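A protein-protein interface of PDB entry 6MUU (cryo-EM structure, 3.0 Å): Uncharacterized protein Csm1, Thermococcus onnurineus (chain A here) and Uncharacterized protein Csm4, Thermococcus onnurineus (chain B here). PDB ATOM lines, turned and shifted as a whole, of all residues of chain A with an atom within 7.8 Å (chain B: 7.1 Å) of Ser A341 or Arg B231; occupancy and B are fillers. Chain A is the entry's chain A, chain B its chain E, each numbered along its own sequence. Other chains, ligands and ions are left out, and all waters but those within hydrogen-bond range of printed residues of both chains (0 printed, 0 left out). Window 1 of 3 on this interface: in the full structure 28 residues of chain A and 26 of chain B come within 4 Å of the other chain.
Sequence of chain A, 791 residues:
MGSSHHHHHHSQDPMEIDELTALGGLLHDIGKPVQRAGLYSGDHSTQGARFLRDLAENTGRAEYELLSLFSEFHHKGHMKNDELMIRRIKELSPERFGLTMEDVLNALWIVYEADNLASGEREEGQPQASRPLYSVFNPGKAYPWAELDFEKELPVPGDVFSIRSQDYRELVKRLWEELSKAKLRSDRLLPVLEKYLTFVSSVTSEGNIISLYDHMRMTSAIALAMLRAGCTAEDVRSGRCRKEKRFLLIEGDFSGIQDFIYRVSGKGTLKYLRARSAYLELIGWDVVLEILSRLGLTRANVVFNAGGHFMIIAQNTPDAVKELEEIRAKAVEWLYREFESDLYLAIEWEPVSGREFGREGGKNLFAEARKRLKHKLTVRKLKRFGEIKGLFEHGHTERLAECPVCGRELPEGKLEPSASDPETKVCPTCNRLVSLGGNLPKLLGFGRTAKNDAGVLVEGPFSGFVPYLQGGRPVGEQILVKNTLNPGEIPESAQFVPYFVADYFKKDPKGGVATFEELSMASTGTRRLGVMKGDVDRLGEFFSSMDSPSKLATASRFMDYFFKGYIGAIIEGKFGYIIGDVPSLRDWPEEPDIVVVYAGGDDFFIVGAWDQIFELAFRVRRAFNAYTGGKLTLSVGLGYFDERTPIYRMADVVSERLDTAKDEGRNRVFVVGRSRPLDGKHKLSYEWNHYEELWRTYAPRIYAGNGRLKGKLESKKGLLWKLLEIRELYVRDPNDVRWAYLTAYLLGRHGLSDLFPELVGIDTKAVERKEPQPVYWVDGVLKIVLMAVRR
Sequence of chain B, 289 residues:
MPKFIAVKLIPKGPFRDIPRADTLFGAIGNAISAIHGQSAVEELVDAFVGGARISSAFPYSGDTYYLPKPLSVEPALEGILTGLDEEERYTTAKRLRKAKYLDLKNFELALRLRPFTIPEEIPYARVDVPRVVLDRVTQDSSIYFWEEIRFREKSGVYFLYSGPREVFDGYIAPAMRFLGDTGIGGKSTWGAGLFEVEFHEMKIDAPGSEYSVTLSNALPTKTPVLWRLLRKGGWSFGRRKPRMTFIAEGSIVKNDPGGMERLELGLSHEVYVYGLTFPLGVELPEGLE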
ATOM      1  N   SER A 255      34.061 -16.589  35.277  1.00  0.00           N
ATOM      2  CA  SER A 255      34.486 -17.469  34.201  1.00  0.00           C
ATOM      3  C   SER A 255      33.635 -17.182  32.973  1.00  0.00           C
ATOM      4  O   SER A 255      32.407 -17.280  33.028  1.00  0.00           O
ATOM      5  CB  SER A 255      34.371 -18.933  34.618  1.00  0.00           C
ATOM      6  OG  SER A 255      34.829 -19.782  33.588  1.00  0.00           O
ATOM      7  N   GLY A 256      34.288 -16.826  31.873  1.00  0.00           N
ATOM      8  CA  GLY A 256      33.584 -16.569  30.636  1.00  0.00           C
ATOM      9  C   GLY A 256      33.448 -15.102  30.304  1.00  0.00           C
ATOM     10  O   GLY A 256      32.397 -14.669  29.834  1.00  0.00           O
ATOM     11  N   ASP A 259      33.826 -14.283  26.351  1.00  0.00           N
ATOM     12  CA  ASP A 259      32.621 -14.724  25.671  1.00  0.00           C
ATOM     13  C   ASP A 259      31.404 -13.906  26.060  1.00  0.00           C
ATOM     14  O   ASP A 259      30.358 -14.032  25.418  1.00  0.00           O
ATOM     15  CB  ASP A 259      32.361 -16.202  25.978  1.00  0.00           C
ATOM     16  CG  ASP A 259      33.415 -17.116  25.380  1.00  0.00           C
ATOM     17  OD1 ASP A 259      33.961 -16.779  24.310  1.00  0.00           O
ATOM     18  OD2 ASP A 259      33.702 -18.170  25.984  1.00  0.00           O
ATOM     19  N   ARG A 263      30.745 -11.116  22.360  1.00  0.00           N
ATOM     20  CA  ARG A 263      29.943 -12.058  21.599  1.00  0.00           C
ATOM     21  C   ARG A 263      29.062 -11.362  20.572  1.00  0.00           C
ATOM     22  O   ARG A 263      28.568 -12.017  19.649  1.00  0.00           O
ATOM     23  CB  ARG A 263      29.070 -12.891  22.554  1.00  0.00           C
ATOM     24  CG  ARG A 263      28.446 -14.146  21.951  1.00  0.00           C
ATOM     25  CD  ARG A 263      27.491 -14.801  22.907  1.00  0.00           C
ATOM     26  NE  ARG A 263      26.753 -15.874  22.256  1.00  0.00           N
ATOM     27  CZ  ARG A 263      25.766 -16.552  22.829  1.00  0.00           C
ATOM     28  NH1 ARG A 263      25.390 -16.261  24.063  1.00  0.00           N
ATOM     29  NH2 ARG A 263      25.144 -17.512  22.161  1.00  0.00           N
ATOM     30  N   LEU A 335      22.511 -15.213  37.658  1.00  0.00           N
ATOM     31  CA  LEU A 335      23.326 -15.235  36.452  1.00  0.00           C
ATOM     32  C   LEU A 335      22.818 -16.237  35.439  1.00  0.00           C
ATOM     33  O   LEU A 335      22.919 -15.988  34.239  1.00  0.00           O
ATOM     34  CB  LEU A 335      24.775 -15.547  36.790  1.00  0.00           C
ATOM     35  CG  LEU A 335      25.634 -14.475  37.437  1.00  0.00           C
ATOM     36  CD1 LEU A 335      26.957 -15.096  37.787  1.00  0.00           C
ATOM     37  CD2 LEU A 335      25.825 -13.326  36.488  1.00  0.00           C
ATOM     38  N   TYR A 336      22.258 -17.361  35.888  1.00  0.00           N
ATOM     39  CA  TYR A 336      21.747 -18.338  34.937  1.00  0.00           C
ATOM     40  C   TYR A 336      20.469 -17.854  34.279  1.00  0.00           C
ATOM     41  O   TYR A 336      20.245 -18.103  33.093  1.00  0.00           O
ATOM     42  CB  TYR A 336      21.507 -19.678  35.616  1.00  0.00           C
ATOM     43  CG  TYR A 336      21.001 -20.702  34.645  1.00  0.00           C
ATOM     44  CD1 TYR A 336      21.821 -21.177  33.640  1.00  0.00           C
ATOM     45  CD2 TYR A 336      19.709 -21.196  34.732  1.00  0.00           C
ATOM     46  CE1 TYR A 336      21.374 -22.102  32.737  1.00  0.00           C
ATOM     47  CE2 TYR A 336      19.248 -22.129  33.833  1.00  0.00           C
ATOM     48  CZ  TYR A 336      20.090 -22.582  32.842  1.00  0.00           C
ATOM     49  OH  TYR A 336      19.644 -23.516  31.939  1.00  0.00           O
ATOM     50  N   ARG A 337      19.625 -17.161  35.032  1.00  0.00           N
ATOM     51  CA  ARG A 337      18.369 -16.679  34.481  1.00  0.00           C
ATOM     52  C   ARG A 337      18.588 -15.514  33.529  1.00  0.00           C
ATOM     53  O   ARG A 337      17.876 -15.391  32.528  1.00  0.00           O
ATOM     54  CB  ARG A 337      17.445 -16.279  35.624  1.00  0.00           C
ATOM     55  CG  ARG A 337      16.042 -15.903  35.226  1.00  0.00           C
ATOM     56  CD  ARG A 337      15.220 -15.590  36.460  1.00  0.00           C
ATOM     57  NE  ARG A 337      15.724 -14.421  37.178  1.00  0.00           N
ATOM     58  CZ  ARG A 337      16.271 -14.465  38.389  1.00  0.00           C
ATOM     59  NH1 ARG A 337      16.695 -13.353  38.965  1.00  0.00           N
ATOM     60  NH2 ARG A 337      16.401 -15.622  39.021  1.00  0.00           N
ATOM     61  N   GLU A 338      19.575 -14.669  33.804  1.00  0.00           N
ATOM     62  CA  GLU A 338      19.786 -13.486  32.984  1.00  0.00           C
ATOM     63  C   GLU A 338      20.678 -13.764  31.784  1.00  0.00           C
ATOM     64  O   GLU A 338      20.334 -13.390  30.661  1.00  0.00           O
ATOM     65  CB  GLU A 338      20.364 -12.361  33.837  1.00  0.00           C
ATOM     66  CG  GLU A 338      19.387 -11.862  34.871  1.00  0.00           C
ATOM     67  CD  GLU A 338      18.194 -11.140  34.267  1.00  0.00           C
ATOM     68  OE1 GLU A 338      18.369 -10.451  33.242  1.00  0.00           O
ATOM     69  OE2 GLU A 338      17.078 -11.266  34.812  1.00  0.00           O
ATOM     70  N   PHE A 339      21.819 -14.408  31.995  1.00  0.00           N
ATOM     71  CA  PHE A 339      22.757 -14.714  30.920  1.00  0.00           C
ATOM     72  C   PHE A 339      22.920 -16.225  30.871  1.00  0.00           C
ATOM     73  O   PHE A 339      23.667 -16.792  31.672  1.00  0.00           O
ATOM     74  CB  PHE A 339      24.091 -14.025  31.150  1.00  0.00           C
ATOM     75  CG  PHE A 339      23.979 -12.551  31.316  1.00  0.00           C
ATOM     76  CD1 PHE A 339      23.709 -11.739  30.233  1.00  0.00           C
ATOM     77  CD2 PHE A 339      24.156 -11.972  32.556  1.00  0.00           C
ATOM     78  CE1 PHE A 339      23.606 -10.376  30.391  1.00  0.00           C
ATOM     79  CE2 PHE A 339      24.056 -10.618  32.716  1.00  0.00           C
ATOM     80  CZ  PHE A 339      23.784  -9.819  31.635  1.00  0.00           C
ATOM     81  N   GLU A 340      22.267 -16.870  29.908  1.00  0.00           N
ATOM     82  CA  GLU A 340      22.121 -18.320  29.930  1.00  0.00           C
ATOM     83  C   GLU A 340      23.444 -19.033  29.679  1.00  0.00           C
ATOM     84  O   GLU A 340      23.817 -19.294  28.530  1.00  0.00           O
ATOM     85  CB  GLU A 340      21.092 -18.754  28.891  1.00  0.00           C
ATOM     86  CG  GLU A 340      19.685 -18.241  29.142  1.00  0.00           C
ATOM     87  CD  GLU A 340      19.030 -18.867  30.356  1.00  0.00           C
ATOM     88  OE1 GLU A 340      19.338 -20.038  30.666  1.00  0.00           O
ATOM     89  OE2 GLU A 340      18.198 -18.192  30.994  1.00  0.00           O
ATOM     90  N   SER A 341      24.143 -19.333  30.777  1.00  0.00           N
ATOM     91  CA  SER A 341      25.405 -20.078  30.818  1.00  0.00           C
ATOM     92  C   SER A 341      26.520 -19.425  30.009  1.00  0.00           C
ATOM     93  O   SER A 341      27.379 -20.118  29.464  1.00  0.00           O
ATOM     94  CB  SER A 341      25.230 -21.530  30.370  1.00  0.00           C
ATOM     95  OG  SER A 341      25.036 -21.604  28.971  1.00  0.00           O
ATOM     96  N   ASP A 342      26.538 -18.099  29.922  1.00  0.00           N
ATOM     97  CA  ASP A 342      27.672 -17.413  29.318  1.00  0.00           C
ATOM     98  C   ASP A 342      28.587 -16.759  30.335  1.00  0.00           C
ATOM     99  O   ASP A 342      29.755 -16.515  30.022  1.00  0.00           O
ATOM    100  CB  ASP A 342      27.203 -16.351  28.321  1.00  0.00           C
ATOM    101  CG  ASP A 342      26.743 -16.948  27.015  1.00  0.00           C
ATOM    102  OD1 ASP A 342      27.244 -18.027  26.638  1.00  0.00           O
ATOM    103  OD2 ASP A 342      25.896 -16.330  26.349  1.00  0.00           O
ATOM    104  N   LEU A 343      28.092 -16.470  31.530  1.00  0.00           N
ATOM    105  CA  LEU A 343      28.890 -15.869  32.583  1.00  0.00           C
ATOM    106  C   LEU A 343      28.587 -16.592  33.882  1.00  0.00           C
ATOM    107  O   LEU A 343      27.421 -16.824  34.203  1.00  0.00           O
ATOM    108  CB  LEU A 343      28.593 -14.381  32.712  1.00  0.00           C
ATOM    109  CG  LEU A 343      29.467 -13.615  33.686  1.00  0.00           C
ATOM    110  CD1 LEU A 343      30.909 -13.670  33.245  1.00  0.00           C
ATOM    111  CD2 LEU A 343      28.982 -12.200  33.771  1.00  0.00           C
ATOM    112  N   TYR A 344      29.633 -16.952  34.617  1.00  0.00           N
ATOM    113  CA  TYR A 344      29.485 -17.711  35.847  1.00  0.00           C
ATOM    114  C   TYR A 344      30.522 -17.279  36.867  1.00  0.00           C
ATOM    115  O   TYR A 344      31.676 -17.028  36.523  1.00  0.00           O
ATOM    116  CB  TYR A 344      29.594 -19.211  35.579  1.00  0.00           C
ATOM    117  CG  TYR A 344      29.675 -20.062  36.818  1.00  0.00           C
ATOM    118  CD1 TYR A 344      28.638 -20.097  37.739  1.00  0.00           C
ATOM    119  CD2 TYR A 344      30.767 -20.884  37.032  1.00  0.00           C
ATOM    120  CE1 TYR A 344      28.720 -20.876  38.867  1.00  0.00           C
ATOM    121  CE2 TYR A 344      30.850 -21.674  38.146  1.00  0.00           C
ATOM    122  CZ  TYR A 344      29.820 -21.674  39.051  1.00  0.00           C
ATOM    123  OH  TYR A 344      29.901 -22.465  40.160  1.00  0.00           O
ATOM    124  N   ARG A 384      29.932 -26.080  36.044  1.00  0.00           N
ATOM    125  CA  ARG A 384      29.667 -24.664  35.824  1.00  0.00           C
ATOM    126  C   ARG A 384      28.329 -24.197  36.364  1.00  0.00           C
ATOM    127  O   ARG A 384      28.227 -23.045  36.761  1.00  0.00           O
ATOM    128  CB  ARG A 384      29.763 -24.286  34.350  1.00  0.00           C
ATOM    129  CG  ARG A 384      31.157 -24.384  33.802  1.00  0.00           C
ATOM    130  CD  ARG A 384      31.304 -23.678  32.461  1.00  0.00           C
ATOM    131  NE  ARG A 384      31.406 -22.226  32.612  1.00  0.00           N
ATOM    132  CZ  ARG A 384      30.479 -21.363  32.222  1.00  0.00           C
ATOM    133  NH1 ARG A 384      29.364 -21.798  31.661  1.00  0.00           N
ATOM    134  NH2 ARG A 384      30.668 -20.064  32.396  1.00  0.00           N
ATOM    135  N   PHE A 385      27.287 -25.004  36.361  1.00  0.00           N
ATOM    136  CA  PHE A 385      26.051 -24.562  36.998  1.00  0.00           C
ATOM    137  C   PHE A 385      25.428 -25.708  37.774  1.00  0.00           C
ATOM    138  O   PHE A 385      24.250 -26.024  37.618  1.00  0.00           O
ATOM    139  CB  PHE A 385      25.086 -23.953  35.986  1.00  0.00           C
ATOM    140  CG  PHE A 385      25.440 -22.550  35.582  1.00  0.00           C
ATOM    141  CD1 PHE A 385      25.061 -21.483  36.371  1.00  0.00           C
ATOM    142  CD2 PHE A 385      26.167 -22.296  34.438  1.00  0.00           C
ATOM    143  CE1 PHE A 385      25.384 -20.194  36.017  1.00  0.00           C
ATOM    144  CE2 PHE A 385      26.503 -21.004  34.093  1.00  0.00           C
ATOM    145  CZ  PHE A 385      26.101 -19.958  34.876  1.00  0.00           C
ATOM    146  N   LEU A 391      19.201 -27.674  35.591  1.00  0.00           N
ATOM    147  CA  LEU A 391      20.201 -27.267  34.618  1.00  0.00           C
ATOM    148  C   LEU A 391      20.143 -28.136  33.376  1.00  0.00           C
ATOM    149  O   LEU A 391      20.370 -27.646  32.266  1.00  0.00           O
ATOM    150  CB  LEU A 391      21.588 -27.306  35.265  1.00  0.00           C
ATOM    151  CG  LEU A 391      22.784 -26.583  34.634  1.00  0.00           C
ATOM    152  CD1 LEU A 391      23.519 -27.369  33.604  1.00  0.00           C
ATOM    153  CD2 LEU A 391      22.311 -25.299  34.014  1.00  0.00           C
ATOM    154  N   LEU A 400       9.815 -19.083  21.351  1.00  0.00           N
ATOM    155  CA  LEU A 400      11.094 -18.580  21.824  1.00  0.00           C
ATOM    156  C   LEU A 400      11.799 -17.882  20.670  1.00  0.00           C
ATOM    157  O   LEU A 400      12.136 -18.520  19.668  1.00  0.00           O
ATOM    158  CB  LEU A 400      11.960 -19.709  22.377  1.00  0.00           C
ATOM    159  CG  LEU A 400      11.497 -20.358  23.678  1.00  0.00           C
ATOM    160  CD1 LEU A 400      12.324 -21.582  23.980  1.00  0.00           C
ATOM    161  CD2 LEU A 400      11.592 -19.376  24.823  1.00  0.00           C
ATOM    162  N   GLY A 407      23.272 -12.974  21.692  1.00  0.00           N
ATOM    163  CA  GLY A 407      22.634 -14.223  21.346  1.00  0.00           C
ATOM    164  C   GLY A 407      21.633 -14.736  22.354  1.00  0.00           C
ATOM    165  O   GLY A 407      21.511 -15.951  22.518  1.00  0.00           O
ATOM    166  N   ARG A 408      20.923 -13.845  23.043  1.00  0.00           N
ATOM    167  CA  ARG A 408      19.961 -14.291  24.040  1.00  0.00           C
ATOM    168  C   ARG A 408      18.762 -14.932  23.373  1.00  0.00           C
ATOM    169  O   ARG A 408      18.316 -14.495  22.312  1.00  0.00           O
ATOM    170  CB  ARG A 408      19.473 -13.139  24.911  1.00  0.00           C
ATOM    171  CG  ARG A 408      20.464 -12.497  25.851  1.00  0.00           C
ATOM    172  CD  ARG A 408      20.755 -13.319  27.101  1.00  0.00           C
ATOM    173  NE  ARG A 408      21.757 -14.352  26.869  1.00  0.00           N
ATOM    174  CZ  ARG A 408      23.067 -14.132  26.816  1.00  0.00           C
ATOM    175  NH1 ARG A 408      23.884 -15.144  26.594  1.00  0.00           N
ATOM    176  NH2 ARG A 408      23.564 -12.914  26.991  1.00  0.00           N
ATOM    177  N   GLU A 409      18.237 -15.971  24.000  1.00  0.00           N
ATOM    178  CA  GLU A 409      17.006 -16.606  23.562  1.00  0.00           C
ATOM    179  C   GLU A 409      15.936 -16.269  24.587  1.00  0.00           C
ATOM    180  O   GLU A 409      15.943 -16.804  25.700  1.00  0.00           O
ATOM    181  CB  GLU A 409      17.172 -18.113  23.434  1.00  0.00           C
ATOM    182  CG  GLU A 409      15.971 -18.758  22.811  1.00  0.00           C
ATOM    183  CD  GLU A 409      16.020 -20.255  22.876  1.00  0.00           C
ATOM    184  OE1 GLU A 409      16.946 -20.777  23.513  1.00  0.00           O
ATOM    185  OE2 GLU A 409      15.132 -20.909  22.295  1.00  0.00           O
ATOM    186  N   ARG B 228      31.723 -29.621  30.766  1.00  0.00           N
ATOM    187  CA  ARG B 228      31.777 -28.329  30.104  1.00  0.00           C
ATOM    188  C   ARG B 228      30.468 -28.145  29.359  1.00  0.00           C
ATOM    189  O   ARG B 228      30.085 -29.003  28.564  1.00  0.00           O
ATOM    190  CB  ARG B 228      32.957 -28.233  29.139  1.00  0.00           C
ATOM    191  CG  ARG B 228      33.114 -26.860  28.525  1.00  0.00           C
ATOM    192  CD  ARG B 228      34.372 -26.723  27.685  1.00  0.00           C
ATOM    193  NE  ARG B 228      34.332 -27.488  26.444  1.00  0.00           N
ATOM    194  CZ  ARG B 228      35.128 -28.515  26.166  1.00  0.00           C
ATOM    195  NH1 ARG B 228      36.033 -28.913  27.048  1.00  0.00           N
ATOM    196  NH2 ARG B 228      35.019 -29.144  25.006  1.00  0.00           N
ATOM    197  N   LEU B 229      29.777 -27.047  29.629  1.00  0.00           N
ATOM    198  CA  LEU B 229      28.453 -26.837  29.067  1.00  0.00           C
ATOM    199  C   LEU B 229      28.578 -26.339  27.641  1.00  0.00           C
ATOM    200  O   LEU B 229      29.120 -25.257  27.401  1.00  0.00           O
ATOM    201  CB  LEU B 229      27.664 -25.835  29.898  1.00  0.00           C
ATOM    202  CG  LEU B 229      27.317 -26.264  31.309  1.00  0.00           C
ATOM    203  CD1 LEU B 229      26.672 -25.113  32.030  1.00  0.00           C
ATOM    204  CD2 LEU B 229      26.393 -27.439  31.241  1.00  0.00           C
ATOM    205  N   LEU B 230      28.065 -27.109  26.702  1.00  0.00           N
ATOM    206  CA  LEU B 230      27.928 -26.668  25.325  1.00  0.00           C
ATOM    207  C   LEU B 230      26.448 -26.386  25.121  1.00  0.00           C
ATOM    208  O   LEU B 230      25.621 -27.297  25.196  1.00  0.00           O
ATOM    209  CB  LEU B 230      28.472 -27.714  24.354  1.00  0.00           C
ATOM    210  CG  LEU B 230      28.629 -27.448  22.856  1.00  0.00           C
ATOM    211  CD1 LEU B 230      27.384 -27.783  22.077  1.00  0.00           C
ATOM    212  CD2 LEU B 230      28.993 -25.999  22.620  1.00  0.00           C
ATOM    213  N   ARG B 231      26.124 -25.125  24.885  1.00  0.00           N
ATOM    214  CA  ARG B 231      24.748 -24.663  24.748  1.00  0.00           C
ATOM    215  C   ARG B 231      24.480 -24.401  23.272  1.00  0.00           C
ATOM    216  O   ARG B 231      24.921 -23.389  22.727  1.00  0.00           O
ATOM    217  CB  ARG B 231      24.539 -23.399  25.570  1.00  0.00           C
ATOM    218  CG  ARG B 231      23.141 -22.872  25.515  1.00  0.00           C
ATOM    219  CD  ARG B 231      22.251 -23.784  26.280  1.00  0.00           C
ATOM    220  NE  ARG B 231      20.856 -23.400  26.178  1.00  0.00           N
ATOM    221  CZ  ARG B 231      20.255 -22.566  27.008  1.00  0.00           C
ATOM    222  NH1 ARG B 231      20.940 -22.030  28.000  1.00  0.00           N
ATOM    223  NH2 ARG B 231      18.975 -22.273  26.846  1.00  0.00           N
ATOM    224  N   LYS B 232      23.751 -25.302  22.618  1.00  0.00           N
ATOM    225  CA  LYS B 232      23.433 -25.111  21.212  1.00  0.00           C
ATOM    226  C   LYS B 232      21.983 -25.470  20.951  1.00  0.00           C
ATOM    227  O   LYS B 232      21.375 -26.264  21.670  1.00  0.00           O
ATOM    228  CB  LYS B 232      24.336 -25.935  20.279  1.00  0.00           C
ATOM    229  CG  LYS B 232      24.055 -27.420  20.256  1.00  0.00           C
ATOM    230  CD  LYS B 232      24.961 -28.151  19.282  1.00  0.00           C
ATOM    231  CE  LYS B 232      24.620 -27.832  17.837  1.00  0.00           C
ATOM    232  NZ  LYS B 232      23.285 -28.358  17.460  1.00  0.00           N
ATOM    233  N   GLY B 233      21.428 -24.842  19.926  1.00  0.00           N
ATOM    234  CA  GLY B 233      20.142 -25.225  19.397  1.00  0.00           C
ATOM    235  C   GLY B 233      20.315 -25.841  18.033  1.00  0.00           C
ATOM    236  O   GLY B 233      21.127 -26.748  17.850  1.00  0.00           O
ATOM    237  N   PRO B 242      15.008 -25.104  19.878  1.00  0.00           N
ATOM    238  CA  PRO B 242      15.412 -24.375  21.082  1.00  0.00           C
ATOM    239  C   PRO B 242      16.803 -24.773  21.536  1.00  0.00           C
ATOM    240  O   PRO B 242      17.257 -25.895  21.308  1.00  0.00           O
ATOM    241  CB  PRO B 242      14.364 -24.791  22.113  1.00  0.00           C
ATOM    242  CG  PRO B 242      13.915 -26.124  21.650  1.00  0.00           C
ATOM    243  CD  PRO B 242      13.927 -26.063  20.162  1.00  0.00           C
ATOM    244  N   ARG B 243      17.484 -23.831  22.182  1.00  0.00           N
ATOM    245  CA  ARG B 243      18.827 -24.080  22.681  1.00  0.00           C
ATOM    246  C   ARG B 243      18.756 -25.047  23.847  1.00  0.00           C
ATOM    247  O   ARG B 243      18.086 -24.771  24.846  1.00  0.00           O
ATOM    248  CB  ARG B 243      19.478 -22.779  23.120  1.00  0.00           C
ATOM    249  CG  ARG B 243      19.727 -21.771  22.035  1.00  0.00           C
ATOM    250  CD  ARG B 243      20.216 -20.496  22.687  1.00  0.00           C
ATOM    251  NE  ARG B 243      20.283 -19.379  21.762  1.00  0.00           N
ATOM    252  CZ  ARG B 243      21.374 -19.025  21.104  1.00  0.00           C
ATOM    253  NH1 ARG B 243      22.497 -19.696  21.283  1.00  0.00           N
ATOM    254  NH2 ARG B 243      21.342 -17.996  20.276  1.00  0.00           N
ATOM    255  N   MET B 244      19.426 -26.180  23.725  1.00  0.00           N
ATOM    256  CA  MET B 244      19.447 -27.171  24.781  1.00  0.00           C
ATOM    257  C   MET B 244      20.830 -27.210  25.406  1.00  0.00           C
ATOM    258  O   MET B 244      21.832 -26.935  24.745  1.00  0.00           O
ATOM    259  CB  MET B 244      19.072 -28.544  24.245  1.00  0.00           C
ATOM    260  CG  MET B 244      17.688 -28.581  23.669  1.00  0.00           C
ATOM    261  SD  MET B 244      17.226 -30.209  23.084  1.00  0.00           S
ATOM    262  CE  MET B 244      17.008 -31.015  24.662  1.00  0.00           C
ATOM    263  N   THR B 245      20.879 -27.536  26.691  1.00  0.00           N
ATOM    264  CA  THR B 245      22.155 -27.659  27.383  1.00  0.00           C
ATOM    265  C   THR B 245      22.686 -29.064  27.155  1.00  0.00           C
ATOM    266  O   THR B 245      22.210 -30.023  27.764  1.00  0.00           O
ATOM    267  CB  THR B 245      22.008 -27.376  28.872  1.00  0.00           C
ATOM    268  OG1 THR B 245      21.172 -28.372  29.461  1.00  0.00           O
ATOM    269  CG2 THR B 245      21.378 -26.029  29.097  1.00  0.00           C
ATOM    270  N   PHE B 246      23.665 -29.183  26.272  1.00  0.00           N
ATOM    271  CA  PHE B 246      24.369 -30.429  26.054  1.00  0.00           C
ATOM    272  C   PHE B 246      25.540 -30.517  27.015  1.00  0.00           C
ATOM    273  O   PHE B 246      25.742 -29.662  27.874  1.00  0.00           O
ATOM    274  CB  PHE B 246      24.862 -30.517  24.616  1.00  0.00           C
ATOM    275  CG  PHE B 246      23.784 -30.742  23.611  1.00  0.00           C
ATOM    276  CD1 PHE B 246      23.399 -32.014  23.260  1.00  0.00           C
ATOM    277  CD2 PHE B 246      23.158 -29.678  23.013  1.00  0.00           C
ATOM    278  CE1 PHE B 246      22.421 -32.212  22.326  1.00  0.00           C
ATOM    279  CE2 PHE B 246      22.170 -29.874  22.090  1.00  0.00           C
ATOM    280  CZ  PHE B 246      21.803 -31.141  21.748  1.00  0.00           C
ATOM    281  N   ILE B 247      26.326 -31.566  26.869  1.00  0.00           N
ATOM    282  CA  ILE B 247      27.587 -31.685  27.568  1.00  0.00           C
ATOM    283  C   ILE B 247      28.647 -31.696  26.473  1.00  0.00           C
ATOM    284  O   ILE B 247      28.363 -32.010  25.315  1.00  0.00           O
ATOM    285  CB  ILE B 247      27.610 -32.951  28.449  1.00  0.00           C
ATOM    286  CG1 ILE B 247      28.394 -32.727  29.714  1.00  0.00           C
ATOM    287  CG2 ILE B 247      28.265 -34.119  27.757  1.00  0.00           C
ATOM    288  CD1 ILE B 247      28.220 -33.856  30.663  1.00  0.00           C
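The backbone carbonyl oxygen of Gly A407 is in hydrogen-bond range of the guanidinium group of Arg B243 (3.0 Å). OE1 of Glu A409 lies close to N of Arg B243 (3.4 Å). The side-chain carboxylate (OE1) of Glu A340 is in salt-bridge range of the guanidinium group (NH1) of Arg B231 (3.7 Å). The backbone carbonyl oxygen of Leu A391 sits at hydrogen-bond distance from the side-chain hydroxyl of Thr B245, at 3.0 Å.
The guanidinium group (NH1) of Arg A263 is in salt-bridge range of the side-chain carboxylate (OD1) of Asp A342, at 3.6 Å. O of Ser A341 sits at hydrogen-bond distance from NH1 of Arg A384, 3.4 Å away. The guanidinium group of Arg A384 lies within hydrogen-bond range of the backbone carbonyl oxygen of Ser A255 (3.3 Å). O of Arg B243 sits at hydrogen-bond distance from NH2 of Arg B231 (3.3 Å).
Among the printed residues, pairs that only touch across the chains: Arg A263 with Arg B243, Glu A409 with Pro B242, Leu A391 with Leu B229, Phe A385 with Leu B229, Ser A341 with Arg B231 and Arg A384 with Leu B229.
Printed residues of chain B within 4 Å of Arg A263: Arg B243. Of the printed residues of chain B, Ser A341 touches Arg B231 (3.9 Å). Arg B231 touches just these residues of chain A: Glu A340 (3.4 Å) and Ser A341 (3.9 Å). Printed residues of chain A within 4 Å of Arg B243: Arg A263, Gly A407 and Glu A409. Printed residues of chain A within 4 Å of Thr B245: Leu A391. The nearest residue of chain A that does not touch Arg B231 is Glu A409 (4.2 Å). The nearest printed residue of chain B that does not touch Glu A409 is Arg B231 (4.2 Å).
Printed residues of chain A that touch a printed residue of chain B: Arg A263, Glu A340, Ser A341, Arg A384, Phe A385, Leu A391, Gly A407 and Glu A409. Hydrophobic or aromatic side chains of chain B within 4 Å of the printed part of chain A: Leu B229 and Pro B242. Among the printed residues, 10 pairs touch across the chains. Among the printed residues, Asp or Glu carboxylates within 4 Å of a Lys or Arg side-chain nitrogen of the other chain: Glu A340 with Arg B231 (3.7 Å).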
